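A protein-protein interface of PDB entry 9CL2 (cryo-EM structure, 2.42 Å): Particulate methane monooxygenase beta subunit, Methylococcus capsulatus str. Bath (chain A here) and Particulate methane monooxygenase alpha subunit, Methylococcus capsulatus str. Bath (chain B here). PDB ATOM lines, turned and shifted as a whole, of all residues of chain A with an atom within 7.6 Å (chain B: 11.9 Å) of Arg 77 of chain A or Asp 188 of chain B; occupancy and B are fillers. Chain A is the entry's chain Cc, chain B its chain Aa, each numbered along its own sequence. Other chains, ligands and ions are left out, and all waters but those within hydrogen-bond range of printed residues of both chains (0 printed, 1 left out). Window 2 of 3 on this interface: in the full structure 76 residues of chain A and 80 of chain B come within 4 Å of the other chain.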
ATOM      1  N   GLN A  71      -0.156  32.876  23.245  1.00  0.00           N
ATOM      2  CA  GLN A  71       0.653  31.957  22.450  1.00  0.00           C
ATOM      3  C   GLN A  71       1.666  31.234  23.325  1.00  0.00           C
ATOM      4  O   GLN A  71       1.801  30.006  23.252  1.00  0.00           O
ATOM      5  CB  GLN A  71       1.362  32.721  21.331  1.00  0.00           C
ATOM      6  CG  GLN A  71       0.583  32.810  20.034  1.00  0.00           C
ATOM      7  CD  GLN A  71       1.389  33.447  18.919  1.00  0.00           C
ATOM      8  OE1 GLN A  71       2.448  34.027  19.159  1.00  0.00           O
ATOM      9  NE2 GLN A  71       0.892  33.341  17.695  1.00  0.00           N
ATOM     10  N   SER A  72       2.375  31.981  24.178  1.00  0.00           N
ATOM     11  CA  SER A  72       3.377  31.380  25.052  1.00  0.00           C
ATOM     12  C   SER A  72       2.774  30.300  25.935  1.00  0.00           C
ATOM     13  O   SER A  72       3.451  29.323  26.273  1.00  0.00           O
ATOM     14  CB  SER A  72       4.033  32.457  25.913  1.00  0.00           C
ATOM     15  OG  SER A  72       3.360  32.599  27.151  1.00  0.00           O
ATOM     16  N   TYR A  73       1.511  30.459  26.325  1.00  0.00           N
ATOM     17  CA  TYR A  73       0.858  29.408  27.099  1.00  0.00           C
ATOM     18  C   TYR A  73       0.401  28.254  26.209  1.00  0.00           C
ATOM     19  O   TYR A  73       0.755  27.092  26.452  1.00  0.00           O
ATOM     20  CB  TYR A  73      -0.323  29.985  27.875  1.00  0.00           C
ATOM     21  CG  TYR A  73      -1.172  28.938  28.560  1.00  0.00           C
ATOM     22  CD1 TYR A  73      -0.658  28.165  29.590  1.00  0.00           C
ATOM     23  CD2 TYR A  73      -2.490  28.726  28.175  1.00  0.00           C
ATOM     24  CE1 TYR A  73      -1.429  27.207  30.218  1.00  0.00           C
ATOM     25  CE2 TYR A  73      -3.269  27.771  28.798  1.00  0.00           C
ATOM     26  CZ  TYR A  73      -2.734  27.017  29.818  1.00  0.00           C
ATOM     27  OH  TYR A  73      -3.509  26.063  30.440  1.00  0.00           O
ATOM     28  N   LEU A  74      -0.384  28.561  25.171  1.00  0.00           N
ATOM     29  CA  LEU A  74      -1.076  27.524  24.413  1.00  0.00           C
ATOM     30  C   LEU A  74      -0.107  26.668  23.609  1.00  0.00           C
ATOM     31  O   LEU A  74      -0.192  25.437  23.636  1.00  0.00           O
ATOM     32  CB  LEU A  74      -2.119  28.161  23.493  1.00  0.00           C
ATOM     33  CG  LEU A  74      -3.427  28.603  24.152  1.00  0.00           C
ATOM     34  CD1 LEU A  74      -4.391  29.155  23.114  1.00  0.00           C
ATOM     35  CD2 LEU A  74      -4.060  27.453  24.919  1.00  0.00           C
ATOM     36  N   TRP A  75       0.815  27.295  22.874  1.00  0.00           N
ATOM     37  CA  TRP A  75       1.741  26.511  22.064  1.00  0.00           C
ATOM     38  C   TRP A  75       2.652  25.661  22.940  1.00  0.00           C
ATOM     39  O   TRP A  75       2.976  24.521  22.587  1.00  0.00           O
ATOM     40  CB  TRP A  75       2.565  27.426  21.161  1.00  0.00           C
ATOM     41  CG  TRP A  75       3.536  26.678  20.304  1.00  0.00           C
ATOM     42  CD1 TRP A  75       4.893  26.645  20.438  1.00  0.00           C
ATOM     43  CD2 TRP A  75       3.224  25.838  19.187  1.00  0.00           C
ATOM     44  NE1 TRP A  75       5.446  25.844  19.469  1.00  0.00           N
ATOM     45  CE2 TRP A  75       4.441  25.337  18.688  1.00  0.00           C
ATOM     46  CE3 TRP A  75       2.033  25.466  18.557  1.00  0.00           C
ATOM     47  CZ2 TRP A  75       4.502  24.482  17.591  1.00  0.00           C
ATOM     48  CZ3 TRP A  75       2.095  24.618  17.468  1.00  0.00           C
ATOM     49  CH2 TRP A  75       3.322  24.136  16.996  1.00  0.00           C
ATOM     50  N   GLU A  76       3.077  26.198  24.085  1.00  0.00           N
ATOM     51  CA  GLU A  76       3.990  25.462  24.949  1.00  0.00           C
ATOM     52  C   GLU A  76       3.299  24.286  25.631  1.00  0.00           C
ATOM     53  O   GLU A  76       3.886  23.204  25.748  1.00  0.00           O
ATOM     54  CB  GLU A  76       4.601  26.399  25.991  1.00  0.00           C
ATOM     55  CG  GLU A  76       5.921  25.918  26.582  1.00  0.00           C
ATOM     56  CD  GLU A  76       6.941  25.515  25.530  1.00  0.00           C
ATOM     57  OE1 GLU A  76       6.986  26.152  24.455  1.00  0.00           O
ATOM     58  OE2 GLU A  76       7.703  24.557  25.778  1.00  0.00           O
ATOM     59  N   ARG A  77       2.059  24.468  26.086  1.00  0.00           N
ATOM     60  CA  ARG A  77       1.418  23.442  26.902  1.00  0.00           C
ATOM     61  C   ARG A  77       0.533  22.485  26.117  1.00  0.00           C
ATOM     62  O   ARG A  77       0.406  21.321  26.510  1.00  0.00           O
ATOM     63  CB  ARG A  77       0.585  24.095  28.011  1.00  0.00           C
ATOM     64  CG  ARG A  77       1.414  24.804  29.071  1.00  0.00           C
ATOM     65  CD  ARG A  77       2.658  24.004  29.433  1.00  0.00           C
ATOM     66  NE  ARG A  77       2.354  22.871  30.299  1.00  0.00           N
ATOM     67  CZ  ARG A  77       2.081  22.965  31.593  1.00  0.00           C
ATOM     68  NH1 ARG A  77       2.071  24.133  32.215  1.00  0.00           N
ATOM     69  NH2 ARG A  77       1.812  21.860  32.282  1.00  0.00           N
ATOM     70  N   TYR A  78      -0.082  22.934  25.022  1.00  0.00           N
ATOM     71  CA  TYR A  78      -1.027  22.119  24.274  1.00  0.00           C
ATOM     72  C   TYR A  78      -0.692  21.991  22.798  1.00  0.00           C
ATOM     73  O   TYR A  78      -1.384  21.246  22.094  1.00  0.00           O
ATOM     74  CB  TYR A  78      -2.446  22.698  24.397  1.00  0.00           C
ATOM     75  CG  TYR A  78      -2.890  22.978  25.811  1.00  0.00           C
ATOM     76  CD1 TYR A  78      -3.455  21.985  26.594  1.00  0.00           C
ATOM     77  CD2 TYR A  78      -2.747  24.244  26.360  1.00  0.00           C
ATOM     78  CE1 TYR A  78      -3.864  22.244  27.887  1.00  0.00           C
ATOM     79  CE2 TYR A  78      -3.149  24.511  27.648  1.00  0.00           C
ATOM     80  CZ  TYR A  78      -3.708  23.509  28.409  1.00  0.00           C
ATOM     81  OH  TYR A  78      -4.111  23.775  29.696  1.00  0.00           O
ATOM     82  N   ARG A  79       0.334  22.692  22.311  1.00  0.00           N
ATOM     83  CA  ARG A  79       0.627  22.780  20.878  1.00  0.00           C
ATOM     84  C   ARG A  79      -0.583  23.291  20.100  1.00  0.00           C
ATOM     85  O   ARG A  79      -0.896  22.807  19.011  1.00  0.00           O
ATOM     86  CB  ARG A  79       1.110  21.437  20.321  1.00  0.00           C
ATOM     87  CG  ARG A  79       2.512  21.047  20.755  1.00  0.00           C
ATOM     88  CD  ARG A  79       3.543  22.034  20.233  1.00  0.00           C
ATOM     89  NE  ARG A  79       4.894  21.688  20.652  1.00  0.00           N
ATOM     90  CZ  ARG A  79       5.461  22.103  21.777  1.00  0.00           C
ATOM     91  NH1 ARG A  79       4.820  22.891  22.624  1.00  0.00           N
ATOM     92  NH2 ARG A  79       6.704  21.720  22.057  1.00  0.00           N
ATOM     93  N   LEU A  80      -1.271  24.285  20.666  1.00  0.00           N
ATOM     94  CA  LEU A  80      -2.416  24.899  20.011  1.00  0.00           C
ATOM     95  C   LEU A  80      -1.990  26.235  19.427  1.00  0.00           C
ATOM     96  O   LEU A  80      -1.684  27.164  20.190  1.00  0.00           O
ATOM     97  CB  LEU A  80      -3.567  25.087  20.996  1.00  0.00           C
ATOM     98  CG  LEU A  80      -4.270  23.808  21.458  1.00  0.00           C
ATOM     99  CD1 LEU A  80      -5.303  24.122  22.527  1.00  0.00           C
ATOM    100  CD2 LEU A  80      -4.903  23.076  20.286  1.00  0.00           C
ATOM    101  N   TYR A 136      10.322  30.773  19.826  1.00  0.00           N
ATOM    102  CA  TYR A 136       9.710  32.027  20.248  1.00  0.00           C
ATOM    103  C   TYR A 136      10.529  33.258  19.882  1.00  0.00           C
ATOM    104  O   TYR A 136       9.952  34.339  19.755  1.00  0.00           O
ATOM    105  CB  TYR A 136       9.449  32.008  21.755  1.00  0.00           C
ATOM    106  CG  TYR A 136       8.284  31.133  22.154  1.00  0.00           C
ATOM    107  CD1 TYR A 136       6.977  31.576  21.999  1.00  0.00           C
ATOM    108  CD2 TYR A 136       8.486  29.864  22.678  1.00  0.00           C
ATOM    109  CE1 TYR A 136       5.905  30.784  22.359  1.00  0.00           C
ATOM    110  CE2 TYR A 136       7.419  29.063  23.040  1.00  0.00           C
ATOM    111  CZ  TYR A 136       6.132  29.529  22.879  1.00  0.00           C
ATOM    112  OH  TYR A 136       5.066  28.737  23.237  1.00  0.00           O
ATOM    113  N   ARG A 231       4.380  33.693  30.517  1.00  0.00           N
ATOM    114  CA  ARG A 231       5.040  32.554  31.145  1.00  0.00           C
ATOM    115  C   ARG A 231       4.912  32.615  32.660  1.00  0.00           C
ATOM    116  O   ARG A 231       4.669  31.593  33.312  1.00  0.00           O
ATOM    117  CB  ARG A 231       6.510  32.501  30.729  1.00  0.00           C
ATOM    118  CG  ARG A 231       6.747  31.836  29.384  1.00  0.00           C
ATOM    119  CD  ARG A 231       6.507  30.338  29.467  1.00  0.00           C
ATOM    120  NE  ARG A 231       7.425  29.585  28.621  1.00  0.00           N
ATOM    121  CZ  ARG A 231       7.182  29.257  27.360  1.00  0.00           C
ATOM    122  NH1 ARG A 231       6.053  29.598  26.761  1.00  0.00           N
ATOM    123  NH2 ARG A 231       8.095  28.567  26.682  1.00  0.00           N
ATOM    124  N   SER A 234       1.362  31.729  33.721  1.00  0.00           N
ATOM    125  CA  SER A 234       0.994  30.327  33.560  1.00  0.00           C
ATOM    126  C   SER A 234       1.511  29.436  34.688  1.00  0.00           C
ATOM    127  O   SER A 234       1.410  28.210  34.585  1.00  0.00           O
ATOM    128  CB  SER A 234       1.497  29.806  32.214  1.00  0.00           C
ATOM    129  OG  SER A 234       1.408  30.805  31.214  1.00  0.00           O
ATOM    130  N   ASN A 235       2.061  30.017  35.753  1.00  0.00           N
ATOM    131  CA  ASN A 235       2.640  29.221  36.828  1.00  0.00           C
ATOM    132  C   ASN A 235       1.563  28.477  37.613  1.00  0.00           C
ATOM    133  O   ASN A 235       0.493  29.020  37.896  1.00  0.00           O
ATOM    134  CB  ASN A 235       3.459  30.117  37.762  1.00  0.00           C
ATOM    135  CG  ASN A 235       2.591  30.931  38.707  1.00  0.00           C
ATOM    136  OD1 ASN A 235       2.170  30.449  39.757  1.00  0.00           O
ATOM    137  ND2 ASN A 235       2.321  32.176  38.332  1.00  0.00           N
ATOM    138  N   GLU A 236       1.842  27.214  37.932  1.00  0.00           N
ATOM    139  CA  GLU A 236       0.959  26.395  38.767  1.00  0.00           C
ATOM    140  C   GLU A 236       1.503  26.311  40.193  1.00  0.00           C
ATOM    141  O   GLU A 236       2.023  25.284  40.633  1.00  0.00           O
ATOM    142  CB  GLU A 236       0.790  25.007  38.156  1.00  0.00           C
ATOM    143  CG  GLU A 236       0.373  25.001  36.698  1.00  0.00           C
ATOM    144  CD  GLU A 236       1.225  24.067  35.863  1.00  0.00           C
ATOM    145  OE1 GLU A 236       2.418  24.372  35.656  1.00  0.00           O
ATOM    146  OE2 GLU A 236       0.706  23.020  35.421  1.00  0.00           O
ATOM    147  N   PRO B 178      -9.349  16.509  19.642  1.00  0.00           N
ATOM    148  CA  PRO B 178      -9.247  16.793  21.079  1.00  0.00           C
ATOM    149  C   PRO B 178      -8.339  17.988  21.325  1.00  0.00           C
ATOM    150  O   PRO B 178      -7.293  18.138  20.691  1.00  0.00           O
ATOM    151  CB  PRO B 178      -8.654  15.504  21.663  1.00  0.00           C
ATOM    152  CG  PRO B 178      -8.644  14.490  20.553  1.00  0.00           C
ATOM    153  CD  PRO B 178      -9.323  15.066  19.357  1.00  0.00           C
ATOM    154  N   ILE B 179      -8.752  18.845  22.256  1.00  0.00           N
ATOM    155  CA  ILE B 179      -8.201  20.190  22.390  1.00  0.00           C
ATOM    156  C   ILE B 179      -7.254  20.301  23.582  1.00  0.00           C
ATOM    157  O   ILE B 179      -6.071  20.602  23.419  1.00  0.00           O
ATOM    158  CB  ILE B 179      -9.328  21.243  22.473  1.00  0.00           C
ATOM    159  CG1 ILE B 179     -10.226  21.166  21.237  1.00  0.00           C
ATOM    160  CG2 ILE B 179      -8.744  22.637  22.633  1.00  0.00           C
ATOM    161  CD1 ILE B 179     -11.332  22.198  21.220  1.00  0.00           C
ATOM    162  N   PHE B 180      -7.759  20.070  24.793  1.00  0.00           N
ATOM    163  CA  PHE B 180      -7.065  20.514  25.996  1.00  0.00           C
ATOM    164  C   PHE B 180      -6.392  19.386  26.767  1.00  0.00           C
ATOM    165  O   PHE B 180      -5.173  19.413  26.950  1.00  0.00           O
ATOM    166  CB  PHE B 180      -8.052  21.260  26.902  1.00  0.00           C
ATOM    167  CG  PHE B 180      -8.396  22.637  26.417  1.00  0.00           C
ATOM    168  CD1 PHE B 180      -7.412  23.602  26.271  1.00  0.00           C
ATOM    169  CD2 PHE B 180      -9.704  22.970  26.108  1.00  0.00           C
ATOM    170  CE1 PHE B 180      -7.727  24.870  25.825  1.00  0.00           C
ATOM    171  CE2 PHE B 180     -10.025  24.237  25.662  1.00  0.00           C
ATOM    172  CZ  PHE B 180      -9.036  25.188  25.521  1.00  0.00           C
ATOM    173  N   ILE B 181      -7.143  18.387  27.219  1.00  0.00           N
ATOM    174  CA  ILE B 181      -6.597  17.407  28.158  1.00  0.00           C
ATOM    175  C   ILE B 181      -5.681  16.410  27.450  1.00  0.00           C
ATOM    176  O   ILE B 181      -4.530  16.241  27.886  1.00  0.00           O
ATOM    177  CB  ILE B 181      -7.719  16.692  28.932  1.00  0.00           C
ATOM    178  CG1 ILE B 181      -8.256  17.598  30.041  1.00  0.00           C
ATOM    179  CG2 ILE B 181      -7.210  15.388  29.526  1.00  0.00           C
ATOM    180  CD1 ILE B 181      -9.174  16.897  31.019  1.00  0.00           C
ATOM    181  N   PRO B 182      -6.118  15.714  26.387  1.00  0.00           N
ATOM    182  CA  PRO B 182      -5.196  14.757  25.748  1.00  0.00           C
ATOM    183  C   PRO B 182      -3.941  15.412  25.198  1.00  0.00           C
ATOM    184  O   PRO B 182      -2.851  14.838  25.306  1.00  0.00           O
ATOM    185  CB  PRO B 182      -6.042  14.126  24.630  1.00  0.00           C
ATOM    186  CG  PRO B 182      -7.441  14.522  24.895  1.00  0.00           C
ATOM    187  CD  PRO B 182      -7.409  15.781  25.679  1.00  0.00           C
ATOM    188  N   ARG B 183      -4.065  16.609  24.622  1.00  0.00           N
ATOM    189  CA  ARG B 183      -2.890  17.305  24.109  1.00  0.00           C
ATOM    190  C   ARG B 183      -1.946  17.699  25.237  1.00  0.00           C
ATOM    191  O   ARG B 183      -0.722  17.590  25.096  1.00  0.00           O
ATOM    192  CB  ARG B 183      -3.318  18.530  23.301  1.00  0.00           C
ATOM    193  CG  ARG B 183      -3.889  18.190  21.934  1.00  0.00           C
ATOM    194  CD  ARG B 183      -4.201  19.438  21.125  1.00  0.00           C
ATOM    195  NE  ARG B 183      -3.023  19.973  20.455  1.00  0.00           N
ATOM    196  CZ  ARG B 183      -2.646  19.644  19.228  1.00  0.00           C
ATOM    197  NH1 ARG B 183      -3.328  18.768  18.507  1.00  0.00           N
ATOM    198  NH2 ARG B 183      -1.559  20.207  18.709  1.00  0.00           N
ATOM    199  N   LEU B 184      -2.495  18.159  26.364  1.00  0.00           N
ATOM    200  CA  LEU B 184      -1.661  18.490  27.515  1.00  0.00           C
ATOM    201  C   LEU B 184      -0.919  17.264  28.028  1.00  0.00           C
ATOM    202  O   LEU B 184       0.276  17.336  28.342  1.00  0.00           O
ATOM    203  CB  LEU B 184      -2.515  19.100  28.625  1.00  0.00           C
ATOM    204  CG  LEU B 184      -1.831  19.404  29.959  1.00  0.00           C
ATOM    205  CD1 LEU B 184      -0.981  20.661  29.857  1.00  0.00           C
ATOM    206  CD2 LEU B 184      -2.863  19.542  31.066  1.00  0.00           C
ATOM    207  N   LEU B 185      -1.612  16.125  28.120  1.00  0.00           N
ATOM    208  CA  LEU B 185      -0.955  14.903  28.573  1.00  0.00           C
ATOM    209  C   LEU B 185       0.128  14.459  27.597  1.00  0.00           C
ATOM    210  O   LEU B 185       1.202  14.014  28.016  1.00  0.00           O
ATOM    211  CB  LEU B 185      -1.986  13.793  28.777  1.00  0.00           C
ATOM    212  CG  LEU B 185      -3.091  14.078  29.794  1.00  0.00           C
ATOM    213  CD1 LEU B 185      -4.123  12.961  29.793  1.00  0.00           C
ATOM    214  CD2 LEU B 185      -2.507  14.273  31.185  1.00  0.00           C
ATOM    215  N   MET B 186      -0.135  14.568  26.292  1.00  0.00           N
ATOM    216  CA  MET B 186       0.866  14.182  25.302  1.00  0.00           C
ATOM    217  C   MET B 186       2.092  15.084  25.368  1.00  0.00           C
ATOM    218  O   MET B 186       3.227  14.608  25.251  1.00  0.00           O
ATOM    219  CB  MET B 186       0.254  14.204  23.901  1.00  0.00           C
ATOM    220  CG  MET B 186      -0.737  13.081  23.643  1.00  0.00           C
ATOM    221  SD  MET B 186       0.030  11.627  22.902  1.00  0.00           S
ATOM    222  CE  MET B 186       0.397  12.238  21.259  1.00  0.00           C
ATOM    223  N   VAL B 187       1.886  16.391  25.546  1.00  0.00           N
ATOM    224  CA  VAL B 187       3.017  17.307  25.680  1.00  0.00           C
ATOM    225  C   VAL B 187       3.806  16.996  26.945  1.00  0.00           C
ATOM    226  O   VAL B 187       5.043  16.996  26.938  1.00  0.00           O
ATOM    227  CB  VAL B 187       2.532  18.769  25.656  1.00  0.00           C
ATOM    228  CG1 VAL B 187       3.673  19.713  25.999  1.00  0.00           C
ATOM    229  CG2 VAL B 187       1.962  19.113  24.293  1.00  0.00           C
ATOM    230  N   ASP B 188       3.106  16.724  28.048  1.00  0.00           N
ATOM    231  CA  ASP B 188       3.789  16.365  29.288  1.00  0.00           C
ATOM    232  C   ASP B 188       4.555  15.056  29.138  1.00  0.00           C
ATOM    233  O   ASP B 188       5.650  14.902  29.689  1.00  0.00           O
ATOM    234  CB  ASP B 188       2.783  16.271  30.435  1.00  0.00           C
ATOM    235  CG  ASP B 188       2.266  17.628  30.869  1.00  0.00           C
ATOM    236  OD1 ASP B 188       2.907  18.645  30.532  1.00  0.00           O
ATOM    237  OD2 ASP B 188       1.220  17.677  31.548  1.00  0.00           O
ATOM    238  N   ALA B 189       3.994  14.103  28.396  1.00  0.00           N
ATOM    239  CA  ALA B 189       4.637  12.814  28.176  1.00  0.00           C
ATOM    240  C   ALA B 189       5.804  12.886  27.201  1.00  0.00           C
ATOM    241  O   ALA B 189       6.524  11.894  27.049  1.00  0.00           O
ATOM    242  CB  ALA B 189       3.612  11.793  27.673  1.00  0.00           C
ATOM    243  N   GLY B 190       6.013  14.025  26.544  1.00  0.00           N
ATOM    244  CA  GLY B 190       7.081  14.164  25.577  1.00  0.00           C
ATOM    245  C   GLY B 190       6.712  13.829  24.151  1.00  0.00           C
ATOM    246  O   GLY B 190       7.610  13.721  23.307  1.00  0.00           O
ATOM    247  N   ARG B 191       5.423  13.660  23.851  1.00  0.00           N
ATOM    248  CA  ARG B 191       4.955  13.350  22.507  1.00  0.00           C
ATOM    249  C   ARG B 191       4.401  14.577  21.791  1.00  0.00           C
ATOM    250  O   ARG B 191       3.436  14.466  21.027  1.00  0.00           O
ATOM    251  CB  ARG B 191       3.902  12.244  22.559  1.00  0.00           C
ATOM    252  CG  ARG B 191       4.361  10.983  23.269  1.00  0.00           C
ATOM    253  CD  ARG B 191       3.809   9.739  22.593  1.00  0.00           C
ATOM    254  NE  ARG B 191       2.740   9.127  23.372  1.00  0.00           N
ATOM    255  CZ  ARG B 191       1.845   8.281  22.880  1.00  0.00           C
ATOM    256  NH1 ARG B 191       1.859   7.924  21.607  1.00  0.00           N
ATOM    257  NH2 ARG B 191       0.911   7.785  23.686  1.00  0.00           N
ATOM    258  N   ALA B 192       4.992  15.751  22.030  1.00  0.00           N
ATOM    259  CA  ALA B 192       4.501  16.973  21.402  1.00  0.00           C
ATOM    260  C   ALA B 192       4.665  16.940  19.888  1.00  0.00           C
ATOM    261  O   ALA B 192       3.787  17.420  19.161  1.00  0.00           O
ATOM    262  CB  ALA B 192       5.220  18.189  21.985  1.00  0.00           C
ATOM    263  N   ASP B 193       5.771  16.375  19.395  1.00  0.00           N
ATOM    264  CA  ASP B 193       6.023  16.337  17.959  1.00  0.00           C
ATOM    265  C   ASP B 193       4.965  15.549  17.199  1.00  0.00           C
ATOM    266  O   ASP B 193       4.810  15.750  15.991  1.00  0.00           O
ATOM    267  CB  ASP B 193       7.405  15.744  17.684  1.00  0.00           C
ATOM    268  CG  ASP B 193       7.506  14.290  18.099  1.00  0.00           C
ATOM    269  OD1 ASP B 193       7.354  14.002  19.304  1.00  0.00           O
ATOM    270  OD2 ASP B 193       7.738  13.435  17.218  1.00  0.00           O
ATOM    271  N   GLU B 194       4.238  14.659  17.874  1.00  0.00           N
ATOM    272  CA  GLU B 194       3.170  13.905  17.233  1.00  0.00           C
ATOM    273  C   GLU B 194       1.887  14.707  17.077  1.00  0.00           C
ATOM    274  O   GLU B 194       0.975  14.254  16.378  1.00  0.00           O
ATOM    275  CB  GLU B 194       2.876  12.630  18.027  1.00  0.00           C
ATOM    276  CG  GLU B 194       4.105  11.974  18.631  1.00  0.00           C
ATOM    277  CD  GLU B 194       3.929  10.481  18.825  1.00  0.00           C
ATOM    278  OE1 GLU B 194       2.848   9.960  18.479  1.00  0.00           O
ATOM    279  OE2 GLU B 194       4.870   9.831  19.326  1.00  0.00           O
ATOM    280  N   LEU B 195       1.789  15.880  17.705  1.00  0.00           N
ATOM    281  CA  LEU B 195       0.561  16.661  17.656  1.00  0.00           C
ATOM    282  C   LEU B 195       0.452  17.531  16.411  1.00  0.00           C
ATOM    283  O   LEU B 195      -0.638  18.046  16.133  1.00  0.00           O
ATOM    284  CB  LEU B 195       0.448  17.535  18.906  1.00  0.00           C
ATOM    285  CG  LEU B 195       0.256  16.784  20.225  1.00  0.00           C
ATOM    286  CD1 LEU B 195       0.217  17.753  21.393  1.00  0.00           C
ATOM    287  CD2 LEU B 195      -1.006  15.939  20.184  1.00  0.00           C
ATOM    288  N   VAL B 196       1.536  17.710  15.661  1.00  0.00           N
ATOM    289  CA  VAL B 196       1.525  18.485  14.426  1.00  0.00           C
ATOM    290  C   VAL B 196       2.101  17.618  13.316  1.00  0.00           C
ATOM    291  O   VAL B 196       3.199  17.067  13.459  1.00  0.00           O
ATOM    292  CB  VAL B 196       2.323  19.796  14.559  1.00  0.00           C
ATOM    293  CG1 VAL B 196       2.262  20.585  13.263  1.00  0.00           C
ATOM    294  CG2 VAL B 196       1.792  20.627  15.718  1.00  0.00           C
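The side-chain hydroxyl (OH) of Tyr 73 of chain A lies within hydrogen-bond range of the side-chain hydroxyl (OH) of Tyr 78 of chain A, 2.5 Å away. NH2 of Arg 231 of chain A lies within salt-bridge range of OE1 of Glu 76 of chain A (3.5 Å). The side-chain hydroxyl of Tyr 136 of chain A sits at hydrogen-bond distance from the backbone NH of Glu 76 of chain A, 3.3 Å away. The backbone carbonyl oxygen (O) of Leu 74 of chain A lies within hydrogen-bond range of the backbone NH (N) of Arg 79 of chain A, at 3.1 Å. The guanidinium group (NH1) of Arg 79 of chain A sits at hydrogen-bond distance from the backbone carbonyl oxygen (O) of Glu 76 of chain A. NH1 of Arg 77 of chain A lies within salt-bridge range of OE1 of Glu 236 of chain A, 3.5 Å away.
The backbone carbonyl oxygen (O) of Tyr 78 of chain A is in hydrogen-bond range of the guanidinium group (NE) of Arg 183 of chain B (2.6 Å). The side-chain carboxylate (OD1) of Asp 188 of chain B is in salt-bridge range of the guanidinium group (NH2) of Arg 77 of chain A. The backbone carbonyl oxygen of Arg 79 of chain A sits at hydrogen-bond distance from the guanidinium group of Arg 183 of chain B.
Of the 19 printed residues of chain B, 8 touch a printed residue of chain A. Of the 15 printed residues of chain A, 5 touch a printed residue of chain B. Hydrophobic or aromatic side chains of chain A within 4 Å of the printed part of chain B: Tyr 78 and Leu 80. Among the printed residues, 13 pairs touch across the chains.
Among the printed residues, merely in contact across the chains: Tyr 78 of chain A with Phe 180 of chain B (3.1 Å), Arg 77 of chain A with Val 187 of chain B (3.4 Å), Tyr 78 of chain A with Leu 184 of chain B (3.5 Å), Glu 76 of chain A with Val 187 of chain B (3.5 Å), Leu 80 of chain A with Arg 183 of chain B (3.6 Å), Arg 77 of chain A with Leu 184 of chain B (3.6 Å), Leu 80 of chain A with Ile 179 of chain B (3.7 Å), Arg 79 of chain A with Ala 192 of chain B (3.8 Å), Tyr 78 of chain A with Leu 195 of chain B (3.9 Å) and Arg 79 of chain A with Leu 195 of chain B (3.9 Å).
No residue of chain B comes within 4 Å of Tyr 73 of chain A. Of chain B, only Val 187 comes within 4 Å of Glu 76 of chain A. Of chain B, only Leu 184, Val 187 and Asp 188 come within 4 Å of Arg 77 of chain A. Of the printed residues of chain B, Leu 80 of chain A touches Ile 179 (3.7 Å) and Arg 183 (3.6 Å). No residue of chain B comes within 4 Å of Ser 234 of chain A. Glu 236 of chain A touches none of the printed residues of chain B. Pro 178 of chain B touches none of the printed residues of chain A. Of the printed residues of chain A, Phe 180 of chain B touches Tyr 78 (3.1 Å). Of the printed residues of chain A, Val 187 of chain B touches Glu 76 and Arg 77. Of the printed residues of chain A, Ala 192 of chain B touches Arg 79. Printed residues of chain A within 4 Å of Leu 195 of chain B: Tyr 78 and Arg 79. The nearest residue of chain A that does not touch Asp 188 of chain B is Glu 236 of chain A (6.6 Å). The nearest printed residue of chain A that does not touch Leu 184 of chain B is Tyr 73 of chain A (6.0 Å).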
